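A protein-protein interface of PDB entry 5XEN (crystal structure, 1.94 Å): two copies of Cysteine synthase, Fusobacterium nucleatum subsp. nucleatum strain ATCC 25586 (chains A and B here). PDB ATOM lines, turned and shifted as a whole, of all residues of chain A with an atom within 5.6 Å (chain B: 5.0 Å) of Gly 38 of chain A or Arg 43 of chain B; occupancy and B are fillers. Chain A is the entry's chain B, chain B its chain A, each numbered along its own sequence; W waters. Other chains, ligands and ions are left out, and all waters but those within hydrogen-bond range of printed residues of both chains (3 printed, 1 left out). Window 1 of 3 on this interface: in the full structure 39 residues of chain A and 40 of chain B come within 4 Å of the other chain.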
ATOM      1  N   LYS A  35      18.461  29.070 -21.746  1.00  0.00           N
ATOM      2  CA  LYS A  35      17.695  28.316 -22.733  1.00  0.00           C
ATOM      3  C   LYS A  35      17.194  27.042 -22.095  1.00  0.00           C
ATOM      4  O   LYS A  35      17.975  26.205 -21.688  1.00  0.00           O
ATOM      5  CB  LYS A  35      18.507  28.005 -23.974  1.00  0.00           C
ATOM      6  CG  LYS A  35      17.591  27.418 -25.079  1.00  0.00           C
ATOM      7  CD  LYS A  35      18.071  27.732 -26.462  1.00  0.00           C
ATOM      8  CE  LYS A  35      17.243  27.070 -27.540  1.00  0.00           C
ATOM      9  NZ  LYS A  35      15.941  27.700 -27.693  1.00  0.00           N
ATOM     10  N   LEU A  36      15.882  26.954 -21.907  1.00  0.00           N
ATOM     11  CA  LEU A  36      15.318  25.909 -21.066  1.00  0.00           C
ATOM     12  C   LEU A  36      14.997  24.661 -21.884  1.00  0.00           C
ATOM     13  O   LEU A  36      13.869  24.467 -22.319  1.00  0.00           O
ATOM     14  CB  LEU A  36      14.066  26.411 -20.324  1.00  0.00           C
ATOM     15  CG  LEU A  36      14.257  27.548 -19.321  1.00  0.00           C
ATOM     16  CD1 LEU A  36      12.889  28.031 -18.823  1.00  0.00           C
ATOM     17  CD2 LEU A  36      15.123  27.109 -18.148  1.00  0.00           C
ATOM     18  N   GLU A  37      15.992  23.805 -22.057  1.00  0.00           N
ATOM     19  CA  GLU A  37      15.814  22.546 -22.794  1.00  0.00           C
ATOM     20  C   GLU A  37      15.005  21.510 -22.053  1.00  0.00           C
ATOM     21  O   GLU A  37      14.536  20.548 -22.672  1.00  0.00           O
ATOM     22  CB  GLU A  37      17.160  21.974 -23.229  1.00  0.00           C
ATOM     23  CG  GLU A  37      17.906  22.923 -24.167  1.00  0.00           C
ATOM     24  CD  GLU A  37      17.250  22.946 -25.542  1.00  0.00           C
ATOM     25  OE1 GLU A  37      17.135  21.864 -26.164  1.00  0.00           O
ATOM     26  OE2 GLU A  37      16.850  24.034 -25.997  1.00  0.00           O
ATOM     27  N   GLY A  38      14.795  21.724 -20.754  1.00  0.00           N
ATOM     28  CA  GLY A  38      13.828  20.974 -19.981  1.00  0.00           C
ATOM     29  C   GLY A  38      12.393  21.122 -20.455  1.00  0.00           C
ATOM     30  O   GLY A  38      11.551  20.304 -20.118  1.00  0.00           O
ATOM     31  N   SER A  39      12.125  22.120 -21.286  1.00  0.00           N
ATOM     32  CA  SER A  39      10.815  22.297 -21.892  1.00  0.00           C
ATOM     33  C   SER A  39      10.478  21.313 -23.008  1.00  0.00           C
ATOM     34  O   SER A  39       9.332  21.228 -23.408  1.00  0.00           O
ATOM     35  CB  SER A  39      10.694  23.697 -22.485  1.00  0.00           C
ATOM     36  OG  SER A  39      10.863  24.643 -21.442  1.00  0.00           O
ATOM     37  N   ASN A  40      11.480  20.675 -23.583  1.00  0.00           N
ATOM     38  CA  ASN A  40      11.250  19.607 -24.576  1.00  0.00           C
ATOM     39  C   ASN A  40      10.358  18.524 -23.957  1.00  0.00           C
ATOM     40  O   ASN A  40      10.353  18.350 -22.752  1.00  0.00           O
ATOM     41  CB  ASN A  40      12.586  18.989 -25.018  1.00  0.00           C
ATOM     42  CG  ASN A  40      13.336  19.855 -26.006  1.00  0.00           C
ATOM     43  OD1 ASN A  40      12.871  20.071 -27.130  1.00  0.00           O
ATOM     44  ND2 ASN A  40      14.504  20.388 -25.590  1.00  0.00           N
ATOM     45  N   ARG A  43      11.975  16.301 -21.705  1.00  0.00           N
ATOM     46  CA  ARG A  43      12.533  17.041 -20.570  1.00  0.00           C
ATOM     47  C   ARG A  43      14.051  17.246 -20.612  1.00  0.00           C
ATOM     48  O   ARG A  43      14.648  17.626 -19.603  1.00  0.00           O
ATOM     49  CB  ARG A  43      12.128  16.429 -19.228  1.00  0.00           C
ATOM     50  CG  ARG A  43      10.622  16.307 -19.061  1.00  0.00           C
ATOM     51  CD  ARG A  43       9.989  17.659 -18.977  1.00  0.00           C
ATOM     52  NE  ARG A  43       8.537  17.534 -18.825  1.00  0.00           N
ATOM     53  CZ  ARG A  43       7.639  18.117 -19.600  1.00  0.00           C
ATOM     54  NH1 ARG A  43       8.026  18.903 -20.608  1.00  0.00           N
ATOM     55  NH2 ARG A  43       6.358  17.975 -19.329  1.00  0.00           N
ATOM     56  N   SER A  44      14.641  17.086 -21.787  1.00  0.00           N
ATOM     57  CA  SER A  44      16.060  17.444 -21.998  1.00  0.00           C
ATOM     58  C   SER A  44      16.332  17.807 -23.428  1.00  0.00           C
ATOM     59  O   SER A  44      15.514  17.512 -24.339  1.00  0.00           O
ATOM     60  CB  SER A  44      17.020  16.359 -21.555  1.00  0.00           C
ATOM     61  OG  SER A  44      17.318  15.420 -22.577  1.00  0.00           O
ATOM     62  N   THR A  45      17.492  18.440 -23.621  1.00  0.00           N
ATOM     63  CA  THR A  45      17.980  18.770 -24.948  1.00  0.00           C
ATOM     64  C   THR A  45      18.203  17.525 -25.818  1.00  0.00           C
ATOM     65  O   THR A  45      18.212  17.630 -27.028  1.00  0.00           O
ATOM     66  CB  THR A  45      19.289  19.618 -24.904  1.00  0.00           C
ATOM     67  OG1 THR A  45      19.371  20.425 -26.079  1.00  0.00           O
ATOM     68  CG2 THR A  45      20.537  18.761 -24.793  1.00  0.00           C
ATOM     69  N   SER A 296      20.450  25.305 -20.399  1.00  0.00           N
ATOM     70  CA  SER A 296      19.984  24.413 -19.341  1.00  0.00           C
ATOM     71  C   SER A 296      19.602  23.093 -19.996  1.00  0.00           C
ATOM     72  O   SER A 296      18.621  23.037 -20.731  1.00  0.00           O
ATOM     73  CB  SER A 296      18.797  24.999 -18.587  1.00  0.00           C
ATOM     74  OG  SER A 296      18.176  24.022 -17.771  1.00  0.00           O
ATOM     75  N   THR A 297      20.383  22.048 -19.742  1.00  0.00           N
ATOM     76  CA  THR A 297      20.217  20.802 -20.511  1.00  0.00           C
ATOM     77  C   THR A 297      18.946  20.028 -20.185  1.00  0.00           C
ATOM     78  O   THR A 297      18.296  19.469 -21.092  1.00  0.00           O
ATOM     79  CB  THR A 297      21.453  19.929 -20.356  1.00  0.00           C
ATOM     80  OG1 THR A 297      22.554  20.662 -20.866  1.00  0.00           O
ATOM     81  CG2 THR A 297      21.346  18.606 -21.101  1.00  0.00           C
ATOM     82  N   ASP A 298      18.580  19.990 -18.906  1.00  0.00           N
ATOM     83  CA  ASP A 298      17.366  19.293 -18.509  1.00  0.00           C
ATOM     84  C   ASP A 298      16.673  19.937 -17.321  1.00  0.00           C
ATOM     85  O   ASP A 298      17.214  20.858 -16.679  1.00  0.00           O
ATOM     86  CB  ASP A 298      17.629  17.785 -18.301  1.00  0.00           C
ATOM     87  CG  ASP A 298      18.316  17.434 -16.990  1.00  0.00           C
ATOM     88  OD1 ASP A 298      18.862  18.341 -16.303  1.00  0.00           O
ATOM     89  OD2 ASP A 298      18.359  16.229 -16.661  1.00  0.00           O
ATOM     90  N   SER A 299      15.454  19.480 -17.053  1.00  0.00           N
ATOM     91  CA  SER A 299      14.737  20.023 -15.919  1.00  0.00           C
ATOM     92  C   SER A 299      15.077  19.233 -14.645  1.00  0.00           C
ATOM     93  O   SER A 299      15.670  18.156 -14.691  1.00  0.00           O
ATOM     94  CB  SER A 299      13.257  19.985 -16.185  1.00  0.00           C
ATOM     95  OG  SER A 299      12.856  18.630 -16.183  1.00  0.00           O
ATOM     96  N   GLU A 301      13.257  17.946 -12.163  1.00  0.00           N
ATOM     97  CA  GLU A 301      12.319  16.930 -11.634  1.00  0.00           C
ATOM     98  C   GLU A 301      12.983  15.604 -11.334  1.00  0.00           C
ATOM     99  O   GLU A 301      12.702  14.952 -10.311  1.00  0.00           O
ATOM    100  CB  GLU A 301      11.123  16.676 -12.613  1.00  0.00           C
ATOM    101  CG  GLU A 301      11.329  16.902 -14.161  1.00  0.00           C
ATOM    102  CD  GLU A 301      12.185  15.866 -14.963  1.00  0.00           C
ATOM    103  OE1 GLU A 301      11.601  14.885 -15.493  1.00  0.00           O
ATOM    104  OE2 GLU A 301      13.410  16.091 -15.142  1.00  0.00           O
ATOM    105  N   GLU B  37      -1.290  20.167 -20.782  1.00  0.00           N
ATOM    106  CA  GLU B  37      -1.026  21.202 -19.781  1.00  0.00           C
ATOM    107  C   GLU B  37       0.223  20.932 -18.943  1.00  0.00           C
ATOM    108  O   GLU B  37       0.705  21.815 -18.259  1.00  0.00           O
ATOM    109  CB  GLU B  37      -2.230  21.422 -18.897  1.00  0.00           C
ATOM    110  CG  GLU B  37      -3.437  21.917 -19.677  1.00  0.00           C
ATOM    111  CD  GLU B  37      -3.281  23.357 -20.088  1.00  0.00           C
ATOM    112  OE1 GLU B  37      -3.061  24.207 -19.193  1.00  0.00           O
ATOM    113  OE2 GLU B  37      -3.387  23.640 -21.304  1.00  0.00           O
ATOM    114  N   GLY B  38       0.747  19.718 -19.030  1.00  0.00           N
ATOM    115  CA  GLY B  38       2.064  19.389 -18.510  1.00  0.00           C
ATOM    116  C   GLY B  38       3.194  20.187 -19.152  1.00  0.00           C
ATOM    117  O   GLY B  38       4.280  20.229 -18.601  1.00  0.00           O
ATOM    118  N   SER B  39       2.938  20.822 -20.301  1.00  0.00           N
ATOM    119  CA  SER B  39       3.902  21.675 -20.964  1.00  0.00           C
ATOM    120  C   SER B  39       4.124  23.003 -20.278  1.00  0.00           C
ATOM    121  O   SER B  39       5.118  23.663 -20.558  1.00  0.00           O
ATOM    122  CB  SER B  39       3.467  21.989 -22.398  1.00  0.00           C
ATOM    123  OG  SER B  39       3.369  20.789 -23.139  1.00  0.00           O
ATOM    124  N   ASN B  40       3.172  23.443 -19.457  1.00  0.00           N
ATOM    125  CA  ASN B  40       3.368  24.616 -18.620  1.00  0.00           C
ATOM    126  C   ASN B  40       4.654  24.489 -17.796  1.00  0.00           C
ATOM    127  O   ASN B  40       5.074  23.388 -17.449  1.00  0.00           O
ATOM    128  CB  ASN B  40       2.179  24.837 -17.660  1.00  0.00           C
ATOM    129  CG  ASN B  40       0.924  25.341 -18.360  1.00  0.00           C
ATOM    130  OD1 ASN B  40      -0.101  24.645 -18.381  1.00  0.00           O
ATOM    131  ND2 ASN B  40       1.000  26.489 -18.971  1.00  0.00           N
ATOM    132  N   PRO B  41       5.250  25.628 -17.409  1.00  0.00           N
ATOM    133  CA  PRO B  41       6.532  25.588 -16.675  1.00  0.00           C
ATOM    134  C   PRO B  41       6.453  24.912 -15.295  1.00  0.00           C
ATOM    135  O   PRO B  41       7.413  24.229 -14.867  1.00  0.00           O
ATOM    136  CB  PRO B  41       6.929  27.080 -16.571  1.00  0.00           C
ATOM    137  CG  PRO B  41       5.650  27.822 -16.772  1.00  0.00           C
ATOM    138  CD  PRO B  41       4.853  26.995 -17.739  1.00  0.00           C
ATOM    139  N   GLY B  42       5.322  25.039 -14.621  1.00  0.00           N
ATOM    140  CA  GLY B  42       5.101  24.311 -13.405  1.00  0.00           C
ATOM    141  C   GLY B  42       4.561  22.894 -13.605  1.00  0.00           C
ATOM    142  O   GLY B  42       4.290  22.209 -12.607  1.00  0.00           O
ATOM    143  N   ARG B  43       4.417  22.465 -14.867  1.00  0.00           N
ATOM    144  CA  ARG B  43       4.045  21.106 -15.266  1.00  0.00           C
ATOM    145  C   ARG B  43       2.580  20.724 -15.049  1.00  0.00           C
ATOM    146  O   ARG B  43       2.243  19.551 -15.090  1.00  0.00           O
ATOM    147  CB  ARG B  43       4.960  20.059 -14.622  1.00  0.00           C
ATOM    148  CG  ARG B  43       6.432  20.270 -14.934  1.00  0.00           C
ATOM    149  CD  ARG B  43       6.681  20.067 -16.381  1.00  0.00           C
ATOM    150  NE  ARG B  43       8.092  20.286 -16.687  1.00  0.00           N
ATOM    151  CZ  ARG B  43       8.553  21.102 -17.618  1.00  0.00           C
ATOM    152  NH1 ARG B  43       7.706  21.811 -18.388  1.00  0.00           N
ATOM    153  NH2 ARG B  43       9.853  21.198 -17.805  1.00  0.00           N
ATOM    154  N   SER B  44       1.728  21.718 -14.845  1.00  0.00           N
ATOM    155  CA  SER B  44       0.279  21.494 -14.792  1.00  0.00           C
ATOM    156  C   SER B  44      -0.497  22.702 -15.264  1.00  0.00           C
ATOM    157  O   SER B  44       0.038  23.829 -15.322  1.00  0.00           O
ATOM    158  CB  SER B  44      -0.183  21.119 -13.387  1.00  0.00           C
ATOM    159  OG  SER B  44      -0.501  22.236 -12.566  1.00  0.00           O
ATOM    160  N   THR B  45      -1.782  22.469 -15.513  1.00  0.00           N
ATOM    161  CA  THR B  45      -2.698  23.530 -15.841  1.00  0.00           C
ATOM    162  C   THR B  45      -2.848  24.555 -14.724  1.00  0.00           C
ATOM    163  O   THR B  45      -3.277  25.689 -14.981  1.00  0.00           O
ATOM    164  CB  THR B  45      -4.093  22.983 -16.252  1.00  0.00           C
ATOM    165  OG1 THR B  45      -4.731  23.900 -17.162  1.00  0.00           O
ATOM    166  CG2 THR B  45      -4.956  22.724 -15.027  1.00  0.00           C
ATOM    167  N   ASP B  47      -0.785  26.278 -13.166  1.00  0.00           N
ATOM    168  CA  ASP B  47      -0.018  27.497 -13.398  1.00  0.00           C
ATOM    169  C   ASP B  47      -0.959  28.653 -13.848  1.00  0.00           C
ATOM    170  O   ASP B  47      -0.757  29.838 -13.469  1.00  0.00           O
ATOM    171  CB  ASP B  47       0.968  27.293 -14.546  1.00  0.00           C
ATOM    172  CG  ASP B  47       2.198  26.482 -14.184  1.00  0.00           C
ATOM    173  OD1 ASP B  47       2.248  25.882 -13.068  1.00  0.00           O
ATOM    174  OD2 ASP B  47       3.116  26.424 -15.037  1.00  0.00           O
ATOM    175  N   THR B 297      -4.202  17.345 -17.461  1.00  0.00           N
ATOM    176  CA  THR B 297      -3.963  18.367 -16.449  1.00  0.00           C
ATOM    177  C   THR B 297      -2.487  18.537 -16.075  1.00  0.00           C
ATOM    178  O   THR B 297      -2.043  19.666 -15.843  1.00  0.00           O
ATOM    179  CB  THR B 297      -4.835  18.119 -15.214  1.00  0.00           C
ATOM    180  OG1 THR B 297      -6.214  18.122 -15.647  1.00  0.00           O
ATOM    181  CG2 THR B 297      -4.624  19.190 -14.139  1.00  0.00           C
ATOM    182  N   ASP B 298      -1.755  17.427 -15.985  1.00  0.00           N
ATOM    183  CA  ASP B 298      -0.343  17.499 -15.626  1.00  0.00           C
ATOM    184  C   ASP B 298       0.465  16.420 -16.266  1.00  0.00           C
ATOM    185  O   ASP B 298      -0.083  15.468 -16.844  1.00  0.00           O
ATOM    186  CB  ASP B 298      -0.113  17.576 -14.089  1.00  0.00           C
ATOM    187  CG  ASP B 298      -0.241  16.262 -13.333  1.00  0.00           C
ATOM    188  OD1 ASP B 298      -0.793  15.280 -13.894  1.00  0.00           O
ATOM    189  OD2 ASP B 298       0.163  16.237 -12.114  1.00  0.00           O
ATOM    190  N   SER B 299       1.788  16.559 -16.172  1.00  0.00           N
ATOM    191  CA  SER B 299       2.658  15.537 -16.739  1.00  0.00           C
ATOM    192  C   SER B 299       2.918  14.461 -15.695  1.00  0.00           C
ATOM    193  O   SER B 299       2.684  14.651 -14.488  1.00  0.00           O
ATOM    194  CB  SER B 299       3.954  16.149 -17.251  1.00  0.00           C
ATOM    195  OG  SER B 299       4.711  16.576 -16.148  1.00  0.00           O
ATOM    196  N   GLU B 301       5.718  12.874 -14.642  1.00  0.00           N
ATOM    197  CA  GLU B 301       7.012  12.696 -13.934  1.00  0.00           C
ATOM    198  C   GLU B 301       6.875  12.666 -12.419  1.00  0.00           C
ATOM    199  O   GLU B 301       7.628  11.982 -11.737  1.00  0.00           O
ATOM    200  CB  GLU B 301       8.067  13.759 -14.267  1.00  0.00           C
ATOM    201  CG  GLU B 301       8.009  14.369 -15.635  1.00  0.00           C
ATOM    202  CD  GLU B 301       7.451  15.777 -15.657  1.00  0.00           C
ATOM    203  OE1 GLU B 301       7.067  16.292 -14.583  1.00  0.00           O
ATOM    204  OE2 GLU B 301       7.412  16.370 -16.752  1.00  0.00           O
ATOM    205  N   LYS B 302       5.899  13.378 -11.871  1.00  0.00           N
ATOM    206  CA  LYS B 302       5.779  13.443 -10.412  1.00  0.00           C
ATOM    207  C   LYS B 302       5.086  12.215  -9.805  1.00  0.00           C
ATOM    208  O   LYS B 302       4.798  12.221  -8.610  1.00  0.00           O
ATOM    209  CB  LYS B 302       5.049  14.709  -9.990  1.00  0.00           C
ATOM    210  CG  LYS B 302       3.567  14.756 -10.321  1.00  0.00           C
ATOM    211  CD  LYS B 302       2.889  16.041  -9.803  1.00  0.00           C
ATOM    212  CE  LYS B 302       3.397  17.293 -10.463  1.00  0.00           C
ATOM    213  NZ  LYS B 302       3.051  17.349 -11.919  1.00  0.00           N
HETATM  214  O   HOH W   1      10.265  13.182 -10.542  1.00  0.00           O
HETATM  215  O   HOH W   2       7.329  22.229 -21.825  1.00  0.00           O
HETATM  216  O   HOH W   3       9.833  24.297 -18.884  1.00  0.00           O
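Gly 38 of chain A touches just one residue of chain B: Arg 43.
Printed residues of chain B within 4 Å of Arg 43 of chain A: Gly 38 (3.2 Å), Arg 43 (3.5 Å), Ser 299 (3.7 Å) and Glu 301 (2.6 Å).
Thr 297 of chain A touches none of the printed residues of chain B.
Printed residues of chain B within 4 Å of Ser 299 of chain A: Arg 43 (3.96 Å).
Of the printed residues of chain B, Glu 301 of chain A touches Glu 301 (3.6 Å).
Of the printed residues of chain A, Gly 38 of chain B touches Arg 43 (3.2 Å).
Of chain A, only Gly 38, Arg 43 and Ser 299 come within 4 Å of Arg 43 of chain B.
Thr 297 of chain B touches none of the printed residues of chain A.
Printed residues of chain A within 4 Å of Glu 301 of chain B: Arg 43 (2.6 Å) and Glu 301 (3.6 Å).
The nearest printed residue of chain B that does not touch Gly 38 of chain A is Glu 301 of chain B (6.6 Å).
Gly 38 of chain A touches Arg 43 of chain B, and with the chains exchanged Arg 43 of chain A touches Gly 38 of chain B.
Arg 43 of chain A touches its own counterpart, Arg 43 of chain B.
Arg 43 of chain A touches Glu 301 of chain B, but with the chains exchanged Glu 301 of chain A does not touch Arg 43 of chain B (5.3 Å).
Glu 301 of chain B touches its own counterpart, Glu 301 of chain A.
11 positions are printed for both chains.
Of the 7 pairs that touch across the chains among the printed residues, 6 have their exchanged pair printed and touching as well.
O of Gly 38 of chain B sits at hydrogen-bond distance from NH2 of Arg 43 of chain A, 3.2 Å away.
The guanidinium group (NH2) of Arg 43 of chain B is in hydrogen-bond range of the backbone carbonyl oxygen (O) of Gly 38 of chain A (3.0 Å).
OE2 of Glu 301 of chain B is in salt-bridge range of NE of Arg 43 of chain A.
The backbone carbonyl oxygen of Asn 40 of chain B sits at hydrogen-bond distance from the guanidinium group of Arg 43 of chain B (3.2 Å).
The backbone NH (N) of Ser 299 of chain B sits at hydrogen-bond distance from the backbone carbonyl oxygen (O) of Arg 43 of chain B (3.2 Å).
OE2 of Glu 301 of chain B lies within hydrogen-bond range of OG of Ser 299 of chain B, 2.8 Å away.
The backbone carbonyl oxygen (O) of Asn 40 of chain A sits at hydrogen-bond distance from the guanidinium group (NH1) of Arg 43 of chain A.
O of Arg 43 of chain A sits at hydrogen-bond distance from N of Ser 299 of chain A, 3.3 Å away.
The side-chain hydroxyl (OG) of Ser 299 of chain A lies within hydrogen-bond range of the side-chain carboxylate (OE2) of Glu 301 of chain A, 2.8 Å away.
Arg 43 of chain B touches Arg 43 of chain A.
Arg 43 of chain A touches Ser 299 of chain B.
Arg 43 of chain B touches Ser 299 of chain A (NH2 to CB, 3.96 Å).
OE1 of Glu 301 of chain A touches CG of Glu 301 of chain B, at 3.6 Å.
Water W2 lies within hydrogen-bond range of O of Ser 39 of chain A (2.7 Å), O of Ser 39 of chain B (2.9 Å) and NH1 of Arg 43 of chain B (3.5 Å).
Water W3 bridges OG of Ser 39 of chain A and NH2 of Arg 43 of chain B.
Water W1 bridges the backbone carbonyl oxygen of Glu 301 of chain A and the backbone carbonyl oxygen of Glu 301 of chain B.
Along chain B the printed residues that touch a printed residue of chain A span positions 38 to 301.
Of the 14 printed residues of chain A, 4 touch a printed residue of chain B.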
